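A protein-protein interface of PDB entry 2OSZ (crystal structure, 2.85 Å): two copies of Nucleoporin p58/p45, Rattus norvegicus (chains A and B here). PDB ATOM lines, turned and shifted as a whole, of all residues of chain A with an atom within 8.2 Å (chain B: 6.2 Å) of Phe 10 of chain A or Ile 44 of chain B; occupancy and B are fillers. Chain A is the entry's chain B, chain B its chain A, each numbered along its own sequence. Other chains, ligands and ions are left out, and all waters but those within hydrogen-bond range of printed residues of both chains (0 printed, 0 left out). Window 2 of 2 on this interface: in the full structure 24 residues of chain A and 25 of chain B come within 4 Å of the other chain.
Phe 10 of chain A touches just these residues of chain B: Ile 44 (3.0 Å), Thr 45 (3.6 Å), Pro 46 (3.3 Å) and Leu 49 (3.9 Å).
Printed residues of chain B within 4 Å of Val 14 of chain A: Ile 44.
Printed residues of chain A within 4 Å of Leu 35 of chain B: Phe 17 (3.1 Å) and Glu 18 (3.5 Å).
Ile 44 of chain B touches just these residues of chain A: Phe 10 (3.0 Å) and Val 14 (3.1 Å).
Asp 48 of chain B touches none of the printed residues of chain A.
The nearest residue of chain B that does not touch Phe 10 of chain A is Gln 47 of chain B (5.5 Å).
The nearest printed residue of chain A that does not touch Ala 52 of chain B is Val 14 of chain A (8.4 Å).
No position is printed for both chains.
OE2 of Glu 18 of chain A sits close to O of Leu 35 of chain B (3.5 Å).
Among the printed residues, pairs that only touch across the chains: Phe 10 of chain A with Ile 44 of chain B, Phe 10 of chain A with Thr 45 of chain B, Phe 10 of chain A with Pro 46 of chain B, Phe 10 of chain A with Leu 49 of chain B, Val 14 of chain A with Ile 44 of chain B, Phe 17 of chain A with Leu 35 of chain B, Phe 17 of chain A with Leu 49 of chain B, Phe 17 of chain A with Ala 52 of chain B and Ile 70 of chain A with Leu 49 of chain B.
OG1 of Thr 45 of chain B sits close to N of Gln 47 of chain B (3.0 Å).
The side-chain hydroxyl of Thr 45 of chain B sits at hydrogen-bond distance from the backbone NH of Asp 48 of chain B.
Of the 20 printed residues of chain A, 5 touch a printed residue of chain B.
Hydrophobic or aromatic side chains of chain A that line the printed part of chain B: Phe 10, Val 14, Phe 17 and Ile 70.
Hydrophobic or aromatic side chains of chain B within 4 Å of the printed part of chain A: Leu 35, Ile 44, Pro 46, Leu 49 and Ala 52.
Among the printed residues, 10 pairs touch across the chains.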
ATOM      1  N   MET A   4      -7.313 -24.481  20.372  1.00  0.00           N
ATOM      2  CA  MET A   4      -6.338 -25.378  19.687  1.00  0.00           C
ATOM      3  C   MET A   4      -5.353 -25.977  20.690  1.00  0.00           C
ATOM      4  O   MET A   4      -5.502 -25.802  21.902  1.00  0.00           O
ATOM      5  CB  MET A   4      -5.582 -24.607  18.595  1.00  0.00           C
ATOM      6  N   ALA A   5      -4.344 -26.678  20.174  1.00  0.00           N
ATOM      7  CA  ALA A   5      -3.337 -27.334  21.003  1.00  0.00           C
ATOM      8  C   ALA A   5      -2.846 -26.466  22.154  1.00  0.00           C
ATOM      9  O   ALA A   5      -2.806 -25.232  22.058  1.00  0.00           O
ATOM     10  CB  ALA A   5      -2.153 -27.775  20.146  1.00  0.00           C
ATOM     11  N   PRO A   6      -2.465 -27.109  23.267  1.00  0.00           N
ATOM     12  CA  PRO A   6      -1.973 -26.390  24.443  1.00  0.00           C
ATOM     13  C   PRO A   6      -0.582 -25.804  24.216  1.00  0.00           C
ATOM     14  O   PRO A   6       0.022 -25.247  25.126  1.00  0.00           O
ATOM     15  CB  PRO A   6      -2.004 -27.460  25.534  1.00  0.00           C
ATOM     16  CG  PRO A   6      -1.708 -28.709  24.778  1.00  0.00           C
ATOM     17  CD  PRO A   6      -2.540 -28.557  23.524  1.00  0.00           C
ATOM     18  N   ALA A   7      -0.074 -25.931  22.996  1.00  0.00           N
ATOM     19  CA  ALA A   7       1.243 -25.397  22.674  1.00  0.00           C
ATOM     20  C   ALA A   7       1.101 -24.121  21.845  1.00  0.00           C
ATOM     21  O   ALA A   7       2.039 -23.333  21.733  1.00  0.00           O
ATOM     22  CB  ALA A   7       2.069 -26.438  21.920  1.00  0.00           C
ATOM     23  N   ASP A   8      -0.078 -23.923  21.266  1.00  0.00           N
ATOM     24  CA  ASP A   8      -0.336 -22.734  20.472  1.00  0.00           C
ATOM     25  C   ASP A   8      -0.886 -21.680  21.411  1.00  0.00           C
ATOM     26  O   ASP A   8      -0.677 -20.484  21.209  1.00  0.00           O
ATOM     27  CB  ASP A   8      -1.367 -23.010  19.377  1.00  0.00           C
ATOM     28  CG  ASP A   8      -0.974 -24.167  18.481  1.00  0.00           C
ATOM     29  OD1 ASP A   8       0.240 -24.301  18.196  1.00  0.00           O
ATOM     30  OD2 ASP A   8      -1.881 -24.929  18.054  1.00  0.00           O
ATOM     31  N   TYR A   9      -1.597 -22.136  22.438  1.00  0.00           N
ATOM     32  CA  TYR A   9      -2.180 -21.238  23.432  1.00  0.00           C
ATOM     33  C   TYR A   9      -1.077 -20.723  24.333  1.00  0.00           C
ATOM     34  O   TYR A   9      -1.086 -19.560  24.724  1.00  0.00           O
ATOM     35  CB  TYR A   9      -3.225 -21.965  24.278  1.00  0.00           C
ATOM     36  CG  TYR A   9      -3.825 -21.104  25.361  1.00  0.00           C
ATOM     37  CD1 TYR A   9      -4.354 -19.851  25.062  1.00  0.00           C
ATOM     38  CD2 TYR A   9      -3.894 -21.553  26.682  1.00  0.00           C
ATOM     39  CE1 TYR A   9      -4.939 -19.069  26.043  1.00  0.00           C
ATOM     40  CE2 TYR A   9      -4.480 -20.777  27.673  1.00  0.00           C
ATOM     41  CZ  TYR A   9      -5.001 -19.537  27.343  1.00  0.00           C
ATOM     42  OH  TYR A   9      -5.600 -18.761  28.308  1.00  0.00           O
ATOM     43  N   PHE A  10      -0.130 -21.597  24.659  1.00  0.00           N
ATOM     44  CA  PHE A  10       0.980 -21.196  25.498  1.00  0.00           C
ATOM     45  C   PHE A  10       1.801 -20.132  24.768  1.00  0.00           C
ATOM     46  O   PHE A  10       2.115 -19.087  25.333  1.00  0.00           O
ATOM     47  CB  PHE A  10       1.871 -22.390  25.845  1.00  0.00           C
ATOM     48  CG  PHE A  10       2.974 -22.048  26.799  1.00  0.00           C
ATOM     49  CD1 PHE A  10       2.680 -21.558  28.069  1.00  0.00           C
ATOM     50  CD2 PHE A  10       4.300 -22.165  26.419  1.00  0.00           C
ATOM     51  CE1 PHE A  10       3.698 -21.184  28.948  1.00  0.00           C
ATOM     52  CE2 PHE A  10       5.327 -21.797  27.285  1.00  0.00           C
ATOM     53  CZ  PHE A  10       5.026 -21.305  28.550  1.00  0.00           C
ATOM     54  N   ARG A  11       2.140 -20.390  23.509  1.00  0.00           N
ATOM     55  CA  ARG A  11       2.914 -19.419  22.750  1.00  0.00           C
ATOM     56  C   ARG A  11       2.180 -18.088  22.711  1.00  0.00           C
ATOM     57  O   ARG A  11       2.814 -17.042  22.700  1.00  0.00           O
ATOM     58  CB  ARG A  11       3.195 -19.915  21.324  1.00  0.00           C
ATOM     59  CG  ARG A  11       4.066 -18.953  20.502  1.00  0.00           C
ATOM     60  CD  ARG A  11       4.734 -19.615  19.278  1.00  0.00           C
ATOM     61  NE  ARG A  11       3.779 -20.294  18.400  1.00  0.00           N
ATOM     62  CZ  ARG A  11       3.480 -21.593  18.460  1.00  0.00           C
ATOM     63  NH1 ARG A  11       2.590 -22.106  17.620  1.00  0.00           N
ATOM     64  NH2 ARG A  11       4.081 -22.384  19.347  1.00  0.00           N
ATOM     65  N   VAL A  12       0.854 -18.111  22.700  1.00  0.00           N
ATOM     66  CA  VAL A  12       0.111 -16.857  22.684  1.00  0.00           C
ATOM     67  C   VAL A  12       0.279 -16.133  24.028  1.00  0.00           C
ATOM     68  O   VAL A  12       0.359 -14.905  24.083  1.00  0.00           O
ATOM     69  CB  VAL A  12      -1.394 -17.088  22.390  1.00  0.00           C
ATOM     70  CG1 VAL A  12      -2.192 -15.831  22.694  1.00  0.00           C
ATOM     71  CG2 VAL A  12      -1.579 -17.443  20.936  1.00  0.00           C
ATOM     72  N   LEU A  13       0.328 -16.898  25.114  1.00  0.00           N
ATOM     73  CA  LEU A  13       0.518 -16.307  26.436  1.00  0.00           C
ATOM     74  C   LEU A  13       1.899 -15.667  26.425  1.00  0.00           C
ATOM     75  O   LEU A  13       2.036 -14.461  26.613  1.00  0.00           O
ATOM     76  CB  LEU A  13       0.468 -17.378  27.530  1.00  0.00           C
ATOM     77  CG  LEU A  13      -0.833 -18.155  27.749  1.00  0.00           C
ATOM     78  CD1 LEU A  13      -0.542 -19.296  28.719  1.00  0.00           C
ATOM     79  CD2 LEU A  13      -1.949 -17.235  28.270  1.00  0.00           C
ATOM     80  N   VAL A  14       2.918 -16.492  26.201  1.00  0.00           N
ATOM     81  CA  VAL A  14       4.297 -16.026  26.145  1.00  0.00           C
ATOM     82  C   VAL A  14       4.391 -14.809  25.230  1.00  0.00           C
ATOM     83  O   VAL A  14       5.205 -13.915  25.444  1.00  0.00           O
ATOM     84  CB  VAL A  14       5.223 -17.144  25.626  1.00  0.00           C
ATOM     85  CG1 VAL A  14       6.586 -16.590  25.279  1.00  0.00           C
ATOM     86  CG2 VAL A  14       5.346 -18.219  26.681  1.00  0.00           C
ATOM     87  N   GLN A  15       3.544 -14.778  24.213  1.00  0.00           N
ATOM     88  CA  GLN A  15       3.524 -13.665  23.279  1.00  0.00           C
ATOM     89  C   GLN A  15       3.144 -12.394  24.034  1.00  0.00           C
ATOM     90  O   GLN A  15       3.825 -11.374  23.914  1.00  0.00           O
ATOM     91  CB  GLN A  15       2.497 -13.933  22.180  1.00  0.00           C
ATOM     92  CG  GLN A  15       3.008 -13.824  20.756  1.00  0.00           C
ATOM     93  CD  GLN A  15       1.956 -14.259  19.750  1.00  0.00           C
ATOM     94  OE1 GLN A  15       0.824 -13.767  19.765  1.00  0.00           O
ATOM     95  NE2 GLN A  15       2.322 -15.185  18.872  1.00  0.00           N
ATOM     96  N   GLN A  16       2.060 -12.462  24.814  1.00  0.00           N
ATOM     97  CA  GLN A  16       1.581 -11.308  25.584  1.00  0.00           C
ATOM     98  C   GLN A  16       2.542 -10.918  26.717  1.00  0.00           C
ATOM     99  O   GLN A  16       2.645  -9.743  27.089  1.00  0.00           O
ATOM    100  CB  GLN A  16       0.178 -11.576  26.154  1.00  0.00           C
ATOM    101  CG  GLN A  16       0.129 -12.492  27.368  1.00  0.00           C
ATOM    102  CD  GLN A  16      -1.249 -12.540  28.014  1.00  0.00           C
ATOM    103  OE1 GLN A  16      -2.218 -13.028  27.420  1.00  0.00           O
ATOM    104  NE2 GLN A  16      -1.344 -12.026  29.237  1.00  0.00           N
ATOM    105  N   PHE A  17       3.243 -11.900  27.264  1.00  0.00           N
ATOM    106  CA  PHE A  17       4.198 -11.621  28.313  1.00  0.00           C
ATOM    107  C   PHE A  17       5.202 -10.623  27.740  1.00  0.00           C
ATOM    108  O   PHE A  17       5.399  -9.543  28.295  1.00  0.00           O
ATOM    109  CB  PHE A  17       4.918 -12.904  28.726  1.00  0.00           C
ATOM    110  CG  PHE A  17       5.970 -12.703  29.787  1.00  0.00           C
ATOM    111  CD1 PHE A  17       5.635 -12.185  31.035  1.00  0.00           C
ATOM    112  CD2 PHE A  17       7.291 -13.070  29.557  1.00  0.00           C
ATOM    113  CE1 PHE A  17       6.601 -12.044  32.035  1.00  0.00           C
ATOM    114  CE2 PHE A  17       8.256 -12.929  30.557  1.00  0.00           C
ATOM    115  CZ  PHE A  17       7.907 -12.417  31.794  1.00  0.00           C
ATOM    116  N   GLU A  18       5.817 -10.976  26.612  1.00  0.00           N
ATOM    117  CA  GLU A  18       6.810 -10.124  25.968  1.00  0.00           C
ATOM    118  C   GLU A  18       6.284  -8.727  25.641  1.00  0.00           C
ATOM    119  O   GLU A  18       6.973  -7.732  25.870  1.00  0.00           O
ATOM    120  CB  GLU A  18       7.349 -10.816  24.710  1.00  0.00           C
ATOM    121  CG  GLU A  18       7.946 -12.193  25.016  1.00  0.00           C
ATOM    122  CD  GLU A  18       8.586 -12.880  23.814  1.00  0.00           C
ATOM    123  OE1 GLU A  18       7.927 -12.976  22.750  1.00  0.00           O
ATOM    124  OE2 GLU A  18       9.749 -13.337  23.949  1.00  0.00           O
ATOM    125  N   ILE A  70      -1.303 -14.312  33.272  1.00  0.00           N
ATOM    126  CA  ILE A  70      -0.527 -15.324  32.563  1.00  0.00           C
ATOM    127  C   ILE A  70      -0.219 -16.496  33.502  1.00  0.00           C
ATOM    128  O   ILE A  70      -0.166 -17.644  33.076  1.00  0.00           O
ATOM    129  CB  ILE A  70       0.794 -14.709  32.051  1.00  0.00           C
ATOM    130  CG1 ILE A  70       0.478 -13.466  31.212  1.00  0.00           C
ATOM    131  CG2 ILE A  70       1.575 -15.717  31.227  1.00  0.00           C
ATOM    132  CD1 ILE A  70       1.675 -12.552  30.976  1.00  0.00           C
ATOM    133  N   ASN A  73      -3.506 -18.674  33.816  1.00  0.00           N
ATOM    134  CA  ASN A  73      -3.668 -19.448  32.603  1.00  0.00           C
ATOM    135  C   ASN A  73      -2.657 -20.597  32.525  1.00  0.00           C
ATOM    136  O   ASN A  73      -3.028 -21.709  32.156  1.00  0.00           O
ATOM    137  CB  ASN A  73      -3.557 -18.547  31.372  1.00  0.00           C
ATOM    138  CG  ASN A  73      -4.814 -17.726  31.137  1.00  0.00           C
ATOM    139  OD1 ASN A  73      -5.932 -18.248  31.191  1.00  0.00           O
ATOM    140  ND2 ASN A  73      -4.640 -16.440  30.862  1.00  0.00           N
ATOM    141  N   VAL A  74      -1.391 -20.365  32.863  1.00  0.00           N
ATOM    142  CA  VAL A  74      -0.457 -21.478  32.811  1.00  0.00           C
ATOM    143  C   VAL A  74      -0.620 -22.387  34.030  1.00  0.00           C
ATOM    144  O   VAL A  74      -0.024 -23.462  34.081  1.00  0.00           O
ATOM    145  CB  VAL A  74       1.042 -21.043  32.716  1.00  0.00           C
ATOM    146  CG1 VAL A  74       1.271 -20.194  31.484  1.00  0.00           C
ATOM    147  CG2 VAL A  74       1.464 -20.322  33.974  1.00  0.00           C
ATOM    148  N   LYS A  75      -1.411 -21.969  35.016  1.00  0.00           N
ATOM    149  CA  LYS A  75      -1.626 -22.807  36.201  1.00  0.00           C
ATOM    150  C   LYS A  75      -2.644 -23.847  35.789  1.00  0.00           C
ATOM    151  O   LYS A  75      -2.528 -25.021  36.124  1.00  0.00           O
ATOM    152  CB  LYS A  75      -2.173 -21.987  37.376  1.00  0.00           C
ATOM    153  CG  LYS A  75      -2.356 -22.789  38.675  1.00  0.00           C
ATOM    154  CD  LYS A  75      -2.603 -21.881  39.887  1.00  0.00           C
ATOM    155  CE  LYS A  75      -3.915 -21.105  39.763  1.00  0.00           C
ATOM    156  NZ  LYS A  75      -4.038 -19.963  40.727  1.00  0.00           N
ATOM    157  N   LEU A  77      -3.252 -24.815  32.678  1.00  0.00           N
ATOM    158  CA  LEU A  77      -2.616 -25.727  31.745  1.00  0.00           C
ATOM    159  C   LEU A  77      -1.793 -26.764  32.500  1.00  0.00           C
ATOM    160  O   LEU A  77      -1.760 -27.927  32.115  1.00  0.00           O
ATOM    161  CB  LEU A  77      -1.726 -24.953  30.768  1.00  0.00           C
ATOM    162  CG  LEU A  77      -2.264 -24.630  29.364  1.00  0.00           C
ATOM    163  CD1 LEU A  77      -3.735 -24.275  29.391  1.00  0.00           C
ATOM    164  CD2 LEU A  77      -1.461 -23.482  28.802  1.00  0.00           C
ATOM    165  N   LEU B  35      14.770 -13.484  26.608  1.00  0.00           N
ATOM    166  CA  LEU B  35      13.489 -14.079  26.227  1.00  0.00           C
ATOM    167  C   LEU B  35      13.296 -14.129  24.712  1.00  0.00           C
ATOM    168  O   LEU B  35      12.728 -15.086  24.178  1.00  0.00           O
ATOM    169  CB  LEU B  35      12.320 -13.307  26.829  1.00  0.00           C
ATOM    170  CG  LEU B  35      11.682 -13.800  28.126  1.00  0.00           C
ATOM    171  CD1 LEU B  35      10.350 -13.093  28.236  1.00  0.00           C
ATOM    172  CD2 LEU B  35      11.469 -15.309  28.128  1.00  0.00           C
ATOM    173  N   GLN B  38      15.761 -17.186  23.213  1.00  0.00           N
ATOM    174  CA  GLN B  38      15.151 -18.501  23.324  1.00  0.00           C
ATOM    175  C   GLN B  38      13.929 -18.659  22.421  1.00  0.00           C
ATOM    176  O   GLN B  38      13.826 -19.644  21.695  1.00  0.00           O
ATOM    177  CB  GLN B  38      14.792 -18.769  24.781  1.00  0.00           C
ATOM    178  CG  GLN B  38      16.003 -19.019  25.666  1.00  0.00           C
ATOM    179  CD  GLN B  38      15.649 -19.221  27.124  1.00  0.00           C
ATOM    180  OE1 GLN B  38      16.379 -19.877  27.872  1.00  0.00           O
ATOM    181  NE2 GLN B  38      14.537 -18.646  27.543  1.00  0.00           N
ATOM    182  N   ALA B  39      13.040 -17.669  22.420  1.00  0.00           N
ATOM    183  CA  ALA B  39      11.834 -17.730  21.596  1.00  0.00           C
ATOM    184  C   ALA B  39      12.116 -17.955  20.113  1.00  0.00           C
ATOM    185  O   ALA B  39      11.735 -18.987  19.554  1.00  0.00           O
ATOM    186  CB  ALA B  39      11.013 -16.464  21.785  1.00  0.00           C
ATOM    187  N   SER B  42      14.314 -21.359  19.539  1.00  0.00           N
ATOM    188  CA  SER B  42      13.520 -22.577  19.745  1.00  0.00           C
ATOM    189  C   SER B  42      12.069 -22.177  20.017  1.00  0.00           C
ATOM    190  O   SER B  42      11.266 -22.004  19.085  1.00  0.00           O
ATOM    191  CB  SER B  42      14.104 -23.363  20.934  1.00  0.00           C
ATOM    192  OG  SER B  42      13.095 -23.961  21.729  1.00  0.00           O
ATOM    193  N   HIS B  43      11.764 -22.034  21.306  1.00  0.00           N
ATOM    194  CA  HIS B  43      10.457 -21.638  21.817  1.00  0.00           C
ATOM    195  C   HIS B  43      10.670 -21.679  23.326  1.00  0.00           C
ATOM    196  O   HIS B  43      11.524 -22.428  23.798  1.00  0.00           O
ATOM    197  CB  HIS B  43       9.345 -22.616  21.379  1.00  0.00           C
ATOM    198  CG  HIS B  43       9.378 -23.935  22.075  1.00  0.00           C
ATOM    199  ND1 HIS B  43      10.405 -24.841  21.925  1.00  0.00           N
ATOM    200  CD2 HIS B  43       8.489 -24.503  22.922  1.00  0.00           C
ATOM    201  CE1 HIS B  43      10.145 -25.915  22.650  1.00  0.00           C
ATOM    202  NE2 HIS B  43       8.987 -25.733  23.263  1.00  0.00           N
ATOM    203  N   ILE B  44       9.924 -20.879  24.082  1.00  0.00           N
ATOM    204  CA  ILE B  44      10.086 -20.864  25.537  1.00  0.00           C
ATOM    205  C   ILE B  44       9.150 -21.877  26.224  1.00  0.00           C
ATOM    206  O   ILE B  44       7.991 -22.042  25.825  1.00  0.00           O
ATOM    207  CB  ILE B  44       9.857 -19.429  26.113  1.00  0.00           C
ATOM    208  CG1 ILE B  44       8.457 -19.310  26.707  1.00  0.00           C
ATOM    209  CG2 ILE B  44      10.001 -18.385  25.006  1.00  0.00           C
ATOM    210  CD1 ILE B  44       8.316 -18.150  27.669  1.00  0.00           C
ATOM    211  N   THR B  45       9.671 -22.548  27.249  1.00  0.00           N
ATOM    212  CA  THR B  45       8.925 -23.561  27.994  1.00  0.00           C
ATOM    213  C   THR B  45       8.173 -22.946  29.174  1.00  0.00           C
ATOM    214  O   THR B  45       8.418 -21.797  29.547  1.00  0.00           O
ATOM    215  CB  THR B  45       9.875 -24.648  28.560  1.00  0.00           C
ATOM    216  OG1 THR B  45      10.509 -24.175  29.756  1.00  0.00           O
ATOM    217  CG2 THR B  45      10.962 -24.975  27.563  1.00  0.00           C
ATOM    218  N   PRO B  46       7.228 -23.692  29.768  1.00  0.00           N
ATOM    219  CA  PRO B  46       6.501 -23.131  30.906  1.00  0.00           C
ATOM    220  C   PRO B  46       7.497 -22.883  32.038  1.00  0.00           C
ATOM    221  O   PRO B  46       7.302 -22.008  32.879  1.00  0.00           O
ATOM    222  CB  PRO B  46       5.503 -24.231  31.243  1.00  0.00           C
ATOM    223  CG  PRO B  46       5.232 -24.836  29.923  1.00  0.00           C
ATOM    224  CD  PRO B  46       6.615 -24.956  29.340  1.00  0.00           C
ATOM    225  N   GLN B  47       8.566 -23.676  32.038  1.00  0.00           N
ATOM    226  CA  GLN B  47       9.627 -23.579  33.036  1.00  0.00           C
ATOM    227  C   GLN B  47      10.388 -22.273  32.821  1.00  0.00           C
ATOM    228  O   GLN B  47      10.748 -21.584  33.782  1.00  0.00           O
ATOM    229  CB  GLN B  47      10.563 -24.792  32.904  1.00  0.00           C
ATOM    230  CG  GLN B  47      11.905 -24.675  33.635  1.00  0.00           C
ATOM    231  CD  GLN B  47      11.776 -24.660  35.155  1.00  0.00           C
ATOM    232  OE1 GLN B  47      12.708 -24.256  35.870  1.00  0.00           O
ATOM    233  NE2 GLN B  47      10.624 -25.106  35.657  1.00  0.00           N
ATOM    234  N   ASP B  48      10.622 -21.937  31.554  1.00  0.00           N
ATOM    235  CA  ASP B  48      11.313 -20.704  31.191  1.00  0.00           C
ATOM    236  C   ASP B  48      10.483 -19.497  31.593  1.00  0.00           C
ATOM    237  O   ASP B  48      10.992 -18.569  32.216  1.00  0.00           O
ATOM    238  CB  ASP B  48      11.561 -20.637  29.685  1.00  0.00           C
ATOM    239  CG  ASP B  48      12.660 -21.564  29.237  1.00  0.00           C
ATOM    240  OD1 ASP B  48      12.899 -21.642  28.011  1.00  0.00           O
ATOM    241  OD2 ASP B  48      13.286 -22.210  30.106  1.00  0.00           O
ATOM    242  N   LEU B  49       9.207 -19.503  31.226  1.00  0.00           N
ATOM    243  CA  LEU B  49       8.327 -18.398  31.565  1.00  0.00           C
ATOM    244  C   LEU B  49       8.277 -18.207  33.081  1.00  0.00           C
ATOM    245  O   LEU B  49       8.091 -17.101  33.578  1.00  0.00           O
ATOM    246  CB  LEU B  49       6.928 -18.672  31.053  1.00  0.00           C
ATOM    247  CG  LEU B  49       6.130 -17.473  30.574  1.00  0.00           C
ATOM    248  CD1 LEU B  49       4.671 -17.847  30.650  1.00  0.00           C
ATOM    249  CD2 LEU B  49       6.393 -16.253  31.430  1.00  0.00           C
ATOM    250  N   ALA B  52      11.632 -16.550  34.246  1.00  0.00           N
ATOM    251  CA  ALA B  52      11.466 -15.187  33.784  1.00  0.00           C
ATOM    252  C   ALA B  52      10.639 -14.404  34.773  1.00  0.00           C
ATOM    253  O   ALA B  52      11.087 -13.380  35.285  1.00  0.00           O
ATOM    254  CB  ALA B  52      10.792 -15.182  32.441  1.00  0.00           C
